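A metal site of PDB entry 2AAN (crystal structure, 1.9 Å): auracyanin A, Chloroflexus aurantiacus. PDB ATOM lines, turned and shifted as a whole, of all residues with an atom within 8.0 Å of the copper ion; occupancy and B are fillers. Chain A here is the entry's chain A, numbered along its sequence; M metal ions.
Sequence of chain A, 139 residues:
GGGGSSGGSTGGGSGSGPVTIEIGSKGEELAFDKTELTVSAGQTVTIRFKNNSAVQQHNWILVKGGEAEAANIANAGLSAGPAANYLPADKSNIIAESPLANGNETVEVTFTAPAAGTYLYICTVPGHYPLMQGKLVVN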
ATOM      1  N   SER A  25      27.608   5.349 -12.984  1.00  0.00           N
ATOM      2  CA  SER A  25      27.842   6.347 -11.963  1.00  0.00           C
ATOM      3  C   SER A  25      29.270   6.879 -12.177  1.00  0.00           C
ATOM      4  O   SER A  25      30.158   6.178 -12.646  1.00  0.00           O
ATOM      5  CB  SER A  25      27.664   5.768 -10.590  1.00  0.00           C
ATOM      6  OG  SER A  25      28.705   4.884 -10.239  1.00  0.00           O
ATOM      7  N   GLU A  29      30.661   9.167  -6.771  1.00  0.00           N
ATOM      8  CA  GLU A  29      29.957  10.452  -6.744  1.00  0.00           C
ATOM      9  C   GLU A  29      28.471  10.269  -7.028  1.00  0.00           C
ATOM     10  O   GLU A  29      28.064   9.288  -7.637  1.00  0.00           O
ATOM     11  CB  GLU A  29      30.516  11.391  -7.813  1.00  0.00           C
ATOM     12  CG  GLU A  29      31.962  11.782  -7.588  1.00  0.00           C
ATOM     13  CD  GLU A  29      32.149  12.574  -6.309  1.00  0.00           C
ATOM     14  OE1 GLU A  29      31.251  13.376  -5.947  1.00  0.00           O
ATOM     15  OE2 GLU A  29      33.208  12.400  -5.664  1.00  0.00           O
ATOM     16  N   LEU A  30      27.691  11.278  -6.648  1.00  0.00           N
ATOM     17  CA  LEU A  30      26.287  11.354  -6.905  1.00  0.00           C
ATOM     18  C   LEU A  30      26.106  12.031  -8.276  1.00  0.00           C
ATOM     19  O   LEU A  30      25.685  13.169  -8.378  1.00  0.00           O
ATOM     20  CB  LEU A  30      25.584  12.115  -5.794  1.00  0.00           C
ATOM     21  CG  LEU A  30      25.201  11.304  -4.550  1.00  0.00           C
ATOM     22  CD1 LEU A  30      26.075  10.119  -4.166  1.00  0.00           C
ATOM     23  CD2 LEU A  30      24.920  12.127  -3.408  1.00  0.00           C
ATOM     24  N   ALA A  31      26.444  11.294  -9.328  1.00  0.00           N
ATOM     25  CA  ALA A  31      26.530  11.819 -10.685  1.00  0.00           C
ATOM     26  C   ALA A  31      26.550  10.638 -11.597  1.00  0.00           C
ATOM     27  O   ALA A  31      27.134   9.594 -11.260  1.00  0.00           O
ATOM     28  CB  ALA A  31      27.818  12.611 -10.882  1.00  0.00           C
ATOM     29  N   PHE A  32      25.934  10.813 -12.760  1.00  0.00           N
ATOM     30  CA  PHE A  32      26.154   9.933 -13.895  1.00  0.00           C
ATOM     31  C   PHE A  32      27.467  10.331 -14.540  1.00  0.00           C
ATOM     32  O   PHE A  32      27.845  11.518 -14.546  1.00  0.00           O
ATOM     33  CB  PHE A  32      25.010  10.019 -14.897  1.00  0.00           C
ATOM     34  CG  PHE A  32      23.683   9.540 -14.370  1.00  0.00           C
ATOM     35  CD1 PHE A  32      22.699  10.445 -14.029  1.00  0.00           C
ATOM     36  CD2 PHE A  32      23.411   8.193 -14.303  1.00  0.00           C
ATOM     37  CE1 PHE A  32      21.447   9.996 -13.576  1.00  0.00           C
ATOM     38  CE2 PHE A  32      22.197   7.734 -13.827  1.00  0.00           C
ATOM     39  CZ  PHE A  32      21.218   8.643 -13.442  1.00  0.00           C
ATOM     40  N   PHE A  49      23.341   0.468 -17.642  1.00  0.00           N
ATOM     41  CA  PHE A  49      23.771   1.312 -16.550  1.00  0.00           C
ATOM     42  C   PHE A  49      24.635   0.519 -15.621  1.00  0.00           C
ATOM     43  O   PHE A  49      24.205  -0.474 -15.064  1.00  0.00           O
ATOM     44  CB  PHE A  49      22.553   1.850 -15.843  1.00  0.00           C
ATOM     45  CG  PHE A  49      22.846   2.679 -14.647  1.00  0.00           C
ATOM     46  CD1 PHE A  49      23.723   3.726 -14.709  1.00  0.00           C
ATOM     47  CD2 PHE A  49      22.227   2.409 -13.434  1.00  0.00           C
ATOM     48  CE1 PHE A  49      23.971   4.538 -13.615  1.00  0.00           C
ATOM     49  CE2 PHE A  49      22.494   3.202 -12.328  1.00  0.00           C
ATOM     50  CZ  PHE A  49      23.400   4.274 -12.423  1.00  0.00           C
ATOM     51  N   ASN A  51      26.720   0.460 -12.290  1.00  0.00           N
ATOM     52  CA  ASN A  51      27.000   1.068 -11.002  1.00  0.00           C
ATOM     53  C   ASN A  51      28.465   0.894 -10.671  1.00  0.00           C
ATOM     54  O   ASN A  51      28.911  -0.206 -10.371  1.00  0.00           O
ATOM     55  CB  ASN A  51      26.132   0.439  -9.892  1.00  0.00           C
ATOM     56  CG  ASN A  51      26.183   1.227  -8.619  1.00  0.00           C
ATOM     57  OD1 ASN A  51      26.996   2.163  -8.502  1.00  0.00           O
ATOM     58  ND2 ASN A  51      25.309   0.915  -7.680  1.00  0.00           N
ATOM     59  N   GLN A  56      26.666   2.305  -3.097  1.00  0.00           N
ATOM     60  CA  GLN A  56      25.526   3.108  -3.402  1.00  0.00           C
ATOM     61  C   GLN A  56      24.643   2.185  -4.182  1.00  0.00           C
ATOM     62  O   GLN A  56      25.146   1.237  -4.814  1.00  0.00           O
ATOM     63  CB  GLN A  56      25.943   4.276  -4.248  1.00  0.00           C
ATOM     64  CG  GLN A  56      26.826   5.243  -3.532  1.00  0.00           C
ATOM     65  CD  GLN A  56      26.062   6.142  -2.593  1.00  0.00           C
ATOM     66  OE1 GLN A  56      24.822   6.128  -2.545  1.00  0.00           O
ATOM     67  NE2 GLN A  56      26.786   6.984  -1.896  1.00  0.00           N
ATOM     68  N   GLN A  57      23.335   2.431  -4.080  1.00  0.00           N
ATOM     69  CA  GLN A  57      22.375   1.975  -5.076  1.00  0.00           C
ATOM     70  C   GLN A  57      22.111   3.162  -5.979  1.00  0.00           C
ATOM     71  O   GLN A  57      22.182   4.275  -5.541  1.00  0.00           O
ATOM     72  CB  GLN A  57      21.069   1.424  -4.450  1.00  0.00           C
ATOM     73  CG  GLN A  57      20.590   2.152  -3.245  1.00  0.00           C
ATOM     74  CD  GLN A  57      19.324   1.625  -2.671  1.00  0.00           C
ATOM     75  OE1 GLN A  57      18.685   0.731  -3.228  1.00  0.00           O
ATOM     76  NE2 GLN A  57      18.931   2.200  -1.549  1.00  0.00           N
ATOM     77  N   HIS A  58      21.795   2.882  -7.228  1.00  0.00           N
ATOM     78  CA  HIS A  58      21.401   3.909  -8.192  1.00  0.00           C
ATOM     79  C   HIS A  58      20.363   3.330  -9.141  1.00  0.00           C
ATOM     80  O   HIS A  58      20.352   2.137  -9.435  1.00  0.00           O
ATOM     81  CB  HIS A  58      22.568   4.323  -9.066  1.00  0.00           C
ATOM     82  CG  HIS A  58      23.696   5.016  -8.350  1.00  0.00           C
ATOM     83  ND1 HIS A  58      23.559   6.271  -7.796  1.00  0.00           N
ATOM     84  CD2 HIS A  58      24.971   4.633  -8.110  1.00  0.00           C
ATOM     85  CE1 HIS A  58      24.711   6.626  -7.243  1.00  0.00           C
ATOM     86  NE2 HIS A  58      25.594   5.667  -7.455  1.00  0.00           N
ATOM     87  N   ASN A  59      19.617   4.235  -9.759  1.00  0.00           N
ATOM     88  CA  ASN A  59      18.845   3.883 -10.944  1.00  0.00           C
ATOM     89  C   ASN A  59      18.975   4.965 -12.015  1.00  0.00           C
ATOM     90  O   ASN A  59      19.657   5.975 -11.817  1.00  0.00           O
ATOM     91  CB  ASN A  59      17.393   3.526 -10.593  1.00  0.00           C
ATOM     92  CG  ASN A  59      16.647   4.624  -9.882  1.00  0.00           C
ATOM     93  OD1 ASN A  59      16.996   5.772  -9.999  1.00  0.00           O
ATOM     94  ND2 ASN A  59      15.599   4.274  -9.113  1.00  0.00           N
ATOM     95  N   TRP A  60      18.361   4.690 -13.153  1.00  0.00           N
ATOM     96  CA  TRP A  60      18.345   5.619 -14.312  1.00  0.00           C
ATOM     97  C   TRP A  60      16.917   5.649 -14.765  1.00  0.00           C
ATOM     98  O   TRP A  60      16.423   4.644 -15.244  1.00  0.00           O
ATOM     99  CB  TRP A  60      19.228   5.109 -15.447  1.00  0.00           C
ATOM    100  CG  TRP A  60      19.320   6.020 -16.639  1.00  0.00           C
ATOM    101  CD1 TRP A  60      20.289   6.924 -16.886  1.00  0.00           C
ATOM    102  CD2 TRP A  60      18.457   6.028 -17.786  1.00  0.00           C
ATOM    103  NE1 TRP A  60      20.047   7.581 -18.071  1.00  0.00           N
ATOM    104  CE2 TRP A  60      18.933   7.040 -18.661  1.00  0.00           C
ATOM    105  CE3 TRP A  60      17.308   5.340 -18.129  1.00  0.00           C
ATOM    106  CZ2 TRP A  60      18.299   7.353 -19.857  1.00  0.00           C
ATOM    107  CZ3 TRP A  60      16.674   5.654 -19.324  1.00  0.00           C
ATOM    108  CH2 TRP A  60      17.191   6.634 -20.188  1.00  0.00           C
ATOM    109  N   LEU A 100      16.717  -1.261 -10.309  1.00  0.00           N
ATOM    110  CA  LEU A 100      17.543  -0.694  -9.280  1.00  0.00           C
ATOM    111  C   LEU A 100      18.884  -1.393  -9.256  1.00  0.00           C
ATOM    112  O   LEU A 100      18.945  -2.602  -9.141  1.00  0.00           O
ATOM    113  CB  LEU A 100      16.872  -0.860  -7.944  1.00  0.00           C
ATOM    114  CG  LEU A 100      17.392  -0.149  -6.711  1.00  0.00           C
ATOM    115  CD1 LEU A 100      17.503   1.338  -6.884  1.00  0.00           C
ATOM    116  CD2 LEU A 100      16.435  -0.419  -5.576  1.00  0.00           C
ATOM    117  N   ALA A 101      19.963  -0.638  -9.326  1.00  0.00           N
ATOM    118  CA  ALA A 101      21.271  -1.272  -9.380  1.00  0.00           C
ATOM    119  C   ALA A 101      21.940  -1.180  -8.016  1.00  0.00           C
ATOM    120  O   ALA A 101      22.172  -0.107  -7.489  1.00  0.00           O
ATOM    121  CB  ALA A 101      22.099  -0.677 -10.437  1.00  0.00           C
ATOM    122  N   ILE A 122      17.213  10.962 -14.340  1.00  0.00           N
ATOM    123  CA  ILE A 122      17.515  11.187 -12.936  1.00  0.00           C
ATOM    124  C   ILE A 122      17.680   9.846 -12.234  1.00  0.00           C
ATOM    125  O   ILE A 122      17.332   8.789 -12.757  1.00  0.00           O
ATOM    126  CB  ILE A 122      16.407  11.994 -12.197  1.00  0.00           C
ATOM    127  CG1 ILE A 122      15.079  11.203 -12.117  1.00  0.00           C
ATOM    128  CG2 ILE A 122      16.157  13.298 -12.913  1.00  0.00           C
ATOM    129  CD1 ILE A 122      13.995  11.847 -11.277  1.00  0.00           C
ATOM    130  N   CYS A 123      18.268   9.906 -11.043  1.00  0.00           N
ATOM    131  CA  CYS A 123      18.246   8.753 -10.145  1.00  0.00           C
ATOM    132  C   CYS A 123      17.333   9.116  -8.994  1.00  0.00           C
ATOM    133  O   CYS A 123      17.468  10.194  -8.452  1.00  0.00           O
ATOM    134  CB  CYS A 123      19.646   8.490  -9.623  1.00  0.00           C
ATOM    135  SG  CYS A 123      19.753   7.270  -8.292  1.00  0.00           S
ATOM    136  N   THR A 124      16.438   8.210  -8.616  1.00  0.00           N
ATOM    137  CA  THR A 124      15.510   8.479  -7.508  1.00  0.00           C
ATOM    138  C   THR A 124      15.903   7.817  -6.182  1.00  0.00           C
ATOM    139  O   THR A 124      15.125   7.802  -5.240  1.00  0.00           O
ATOM    140  CB  THR A 124      14.087   8.032  -7.890  1.00  0.00           C
ATOM    141  OG1 THR A 124      14.080   6.633  -8.126  1.00  0.00           O
ATOM    142  CG2 THR A 124      13.638   8.753  -9.146  1.00  0.00           C
ATOM    143  N   VAL A 125      17.121   7.314  -6.066  1.00  0.00           N
ATOM    144  CA  VAL A 125      17.584   6.817  -4.771  1.00  0.00           C
ATOM    145  C   VAL A 125      17.626   8.030  -3.805  1.00  0.00           C
ATOM    146  O   VAL A 125      18.045   9.110  -4.191  1.00  0.00           O
ATOM    147  CB  VAL A 125      18.930   6.070  -4.951  1.00  0.00           C
ATOM    148  CG1 VAL A 125      19.666   5.848  -3.577  1.00  0.00           C
ATOM    149  CG2 VAL A 125      18.700   4.753  -5.728  1.00  0.00           C
ATOM    150  N   PRO A 126      17.119   7.848  -2.564  1.00  0.00           N
ATOM    151  CA  PRO A 126      17.002   8.964  -1.643  1.00  0.00           C
ATOM    152  C   PRO A 126      18.238   9.843  -1.584  1.00  0.00           C
ATOM    153  O   PRO A 126      19.327   9.349  -1.335  1.00  0.00           O
ATOM    154  CB  PRO A 126      16.757   8.258  -0.278  1.00  0.00           C
ATOM    155  CG  PRO A 126      15.913   7.098  -0.662  1.00  0.00           C
ATOM    156  CD  PRO A 126      16.520   6.634  -1.991  1.00  0.00           C
ATOM    157  N   GLY A 127      18.057  11.139  -1.805  1.00  0.00           N
ATOM    158  CA  GLY A 127      19.150  12.099  -1.705  1.00  0.00           C
ATOM    159  C   GLY A 127      20.026  12.283  -2.949  1.00  0.00           C
ATOM    160  O   GLY A 127      20.849  13.204  -2.981  1.00  0.00           O
ATOM    161  N   HIS A 128      19.897  11.441  -3.964  1.00  0.00           N
ATOM    162  CA  HIS A 128      20.828  11.569  -5.133  1.00  0.00           C
ATOM    163  C   HIS A 128      20.438  12.665  -6.104  1.00  0.00           C
ATOM    164  O   HIS A 128      21.306  13.369  -6.619  1.00  0.00           O
ATOM    165  CB  HIS A 128      20.969  10.249  -5.854  1.00  0.00           C
ATOM    166  CG  HIS A 128      21.654   9.224  -5.033  1.00  0.00           C
ATOM    167  ND1 HIS A 128      22.141   8.046  -5.558  1.00  0.00           N
ATOM    168  CD2 HIS A 128      21.942   9.192  -3.699  1.00  0.00           C
ATOM    169  CE1 HIS A 128      22.701   7.344  -4.578  1.00  0.00           C
ATOM    170  NE2 HIS A 128      22.615   8.034  -3.462  1.00  0.00           N
ATOM    171  N   TYR A 129      19.134  12.799  -6.346  1.00  0.00           N
ATOM    172  CA  TYR A 129      18.582  13.957  -7.059  1.00  0.00           C
ATOM    173  C   TYR A 129      18.487  15.044  -6.007  1.00  0.00           C
ATOM    174  O   TYR A 129      18.106  14.746  -4.865  1.00  0.00           O
ATOM    175  CB  TYR A 129      17.207  13.617  -7.681  1.00  0.00           C
ATOM    176  CG  TYR A 129      16.576  14.799  -8.391  1.00  0.00           C
ATOM    177  CD1 TYR A 129      16.926  15.114  -9.693  1.00  0.00           C
ATOM    178  CD2 TYR A 129      15.770  15.697  -7.700  1.00  0.00           C
ATOM    179  CE1 TYR A 129      16.452  16.215 -10.333  1.00  0.00           C
ATOM    180  CE2 TYR A 129      15.268  16.850  -8.337  1.00  0.00           C
ATOM    181  CZ  TYR A 129      15.593  17.094  -9.666  1.00  0.00           C
ATOM    182  OH  TYR A 129      15.121  18.190 -10.356  1.00  0.00           O
ATOM    183  N   MET A 132      22.117  14.182  -9.139  1.00  0.00           N
ATOM    184  CA  MET A 132      22.331  13.101 -10.066  1.00  0.00           C
ATOM    185  C   MET A 132      21.272  13.204 -11.161  1.00  0.00           C
ATOM    186  O   MET A 132      20.145  12.675 -11.073  1.00  0.00           O
ATOM    187  CB  MET A 132      22.325  11.794  -9.301  1.00  0.00           C
ATOM    188  CG  MET A 132      22.895  10.645 -10.110  1.00  0.00           C
ATOM    189  SD  MET A 132      23.308   9.228  -9.124  1.00  0.00           S
ATOM    190  CE  MET A 132      23.628   8.053 -10.461  1.00  0.00           C
HETATM  191 CU    CU M   1      21.822   7.340  -7.498  1.00  0.00          CU
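Residues that only touch the copper ion: Gln 57 (3.7 Å).
Five residues have an atom within 4 Å of the copper ion: Gln 57, His 58, Cys 123, His 128 and Met 132.
Along chain A the residues within 4 Å of the copper ion span positions 57 to 132.
The side-chain sulfur (SD) of Met 132 lies close to the backbone NH (N) of Ala 31 (3.8 Å).
SG of Cys 123 lies close to N of Val 125 (3.4 Å).
SD of Met 132 sits close to ND1 of His 58, 3.3 Å away.
The side-chain sulfur of Cys 123 lies close to the backbone NH of Asn 59 (3.4 Å).
O of Met 132 lies within hydrogen-bond range of N of Cys 123, at 3.3 Å.
The backbone carbonyl oxygen (O) of His 58 lies within hydrogen-bond range of the backbone NH (N) of Ala 101 (2.8 Å).
A ring nitrogen (NE2) of His 128 is in hydrogen-bond range of the side-chain amide oxygen of Gln 56 (3.1 Å).
The copper ion is bound by ND1 of His 58 (2.1 Å), ND1 of His 128 (2.1 Å) and SG of Cys 123 (2.2 Å).
The copper ion has three donor atoms within binding distance.
Slightly farther from the copper ion lies SD of Met 132 (2.9 Å).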
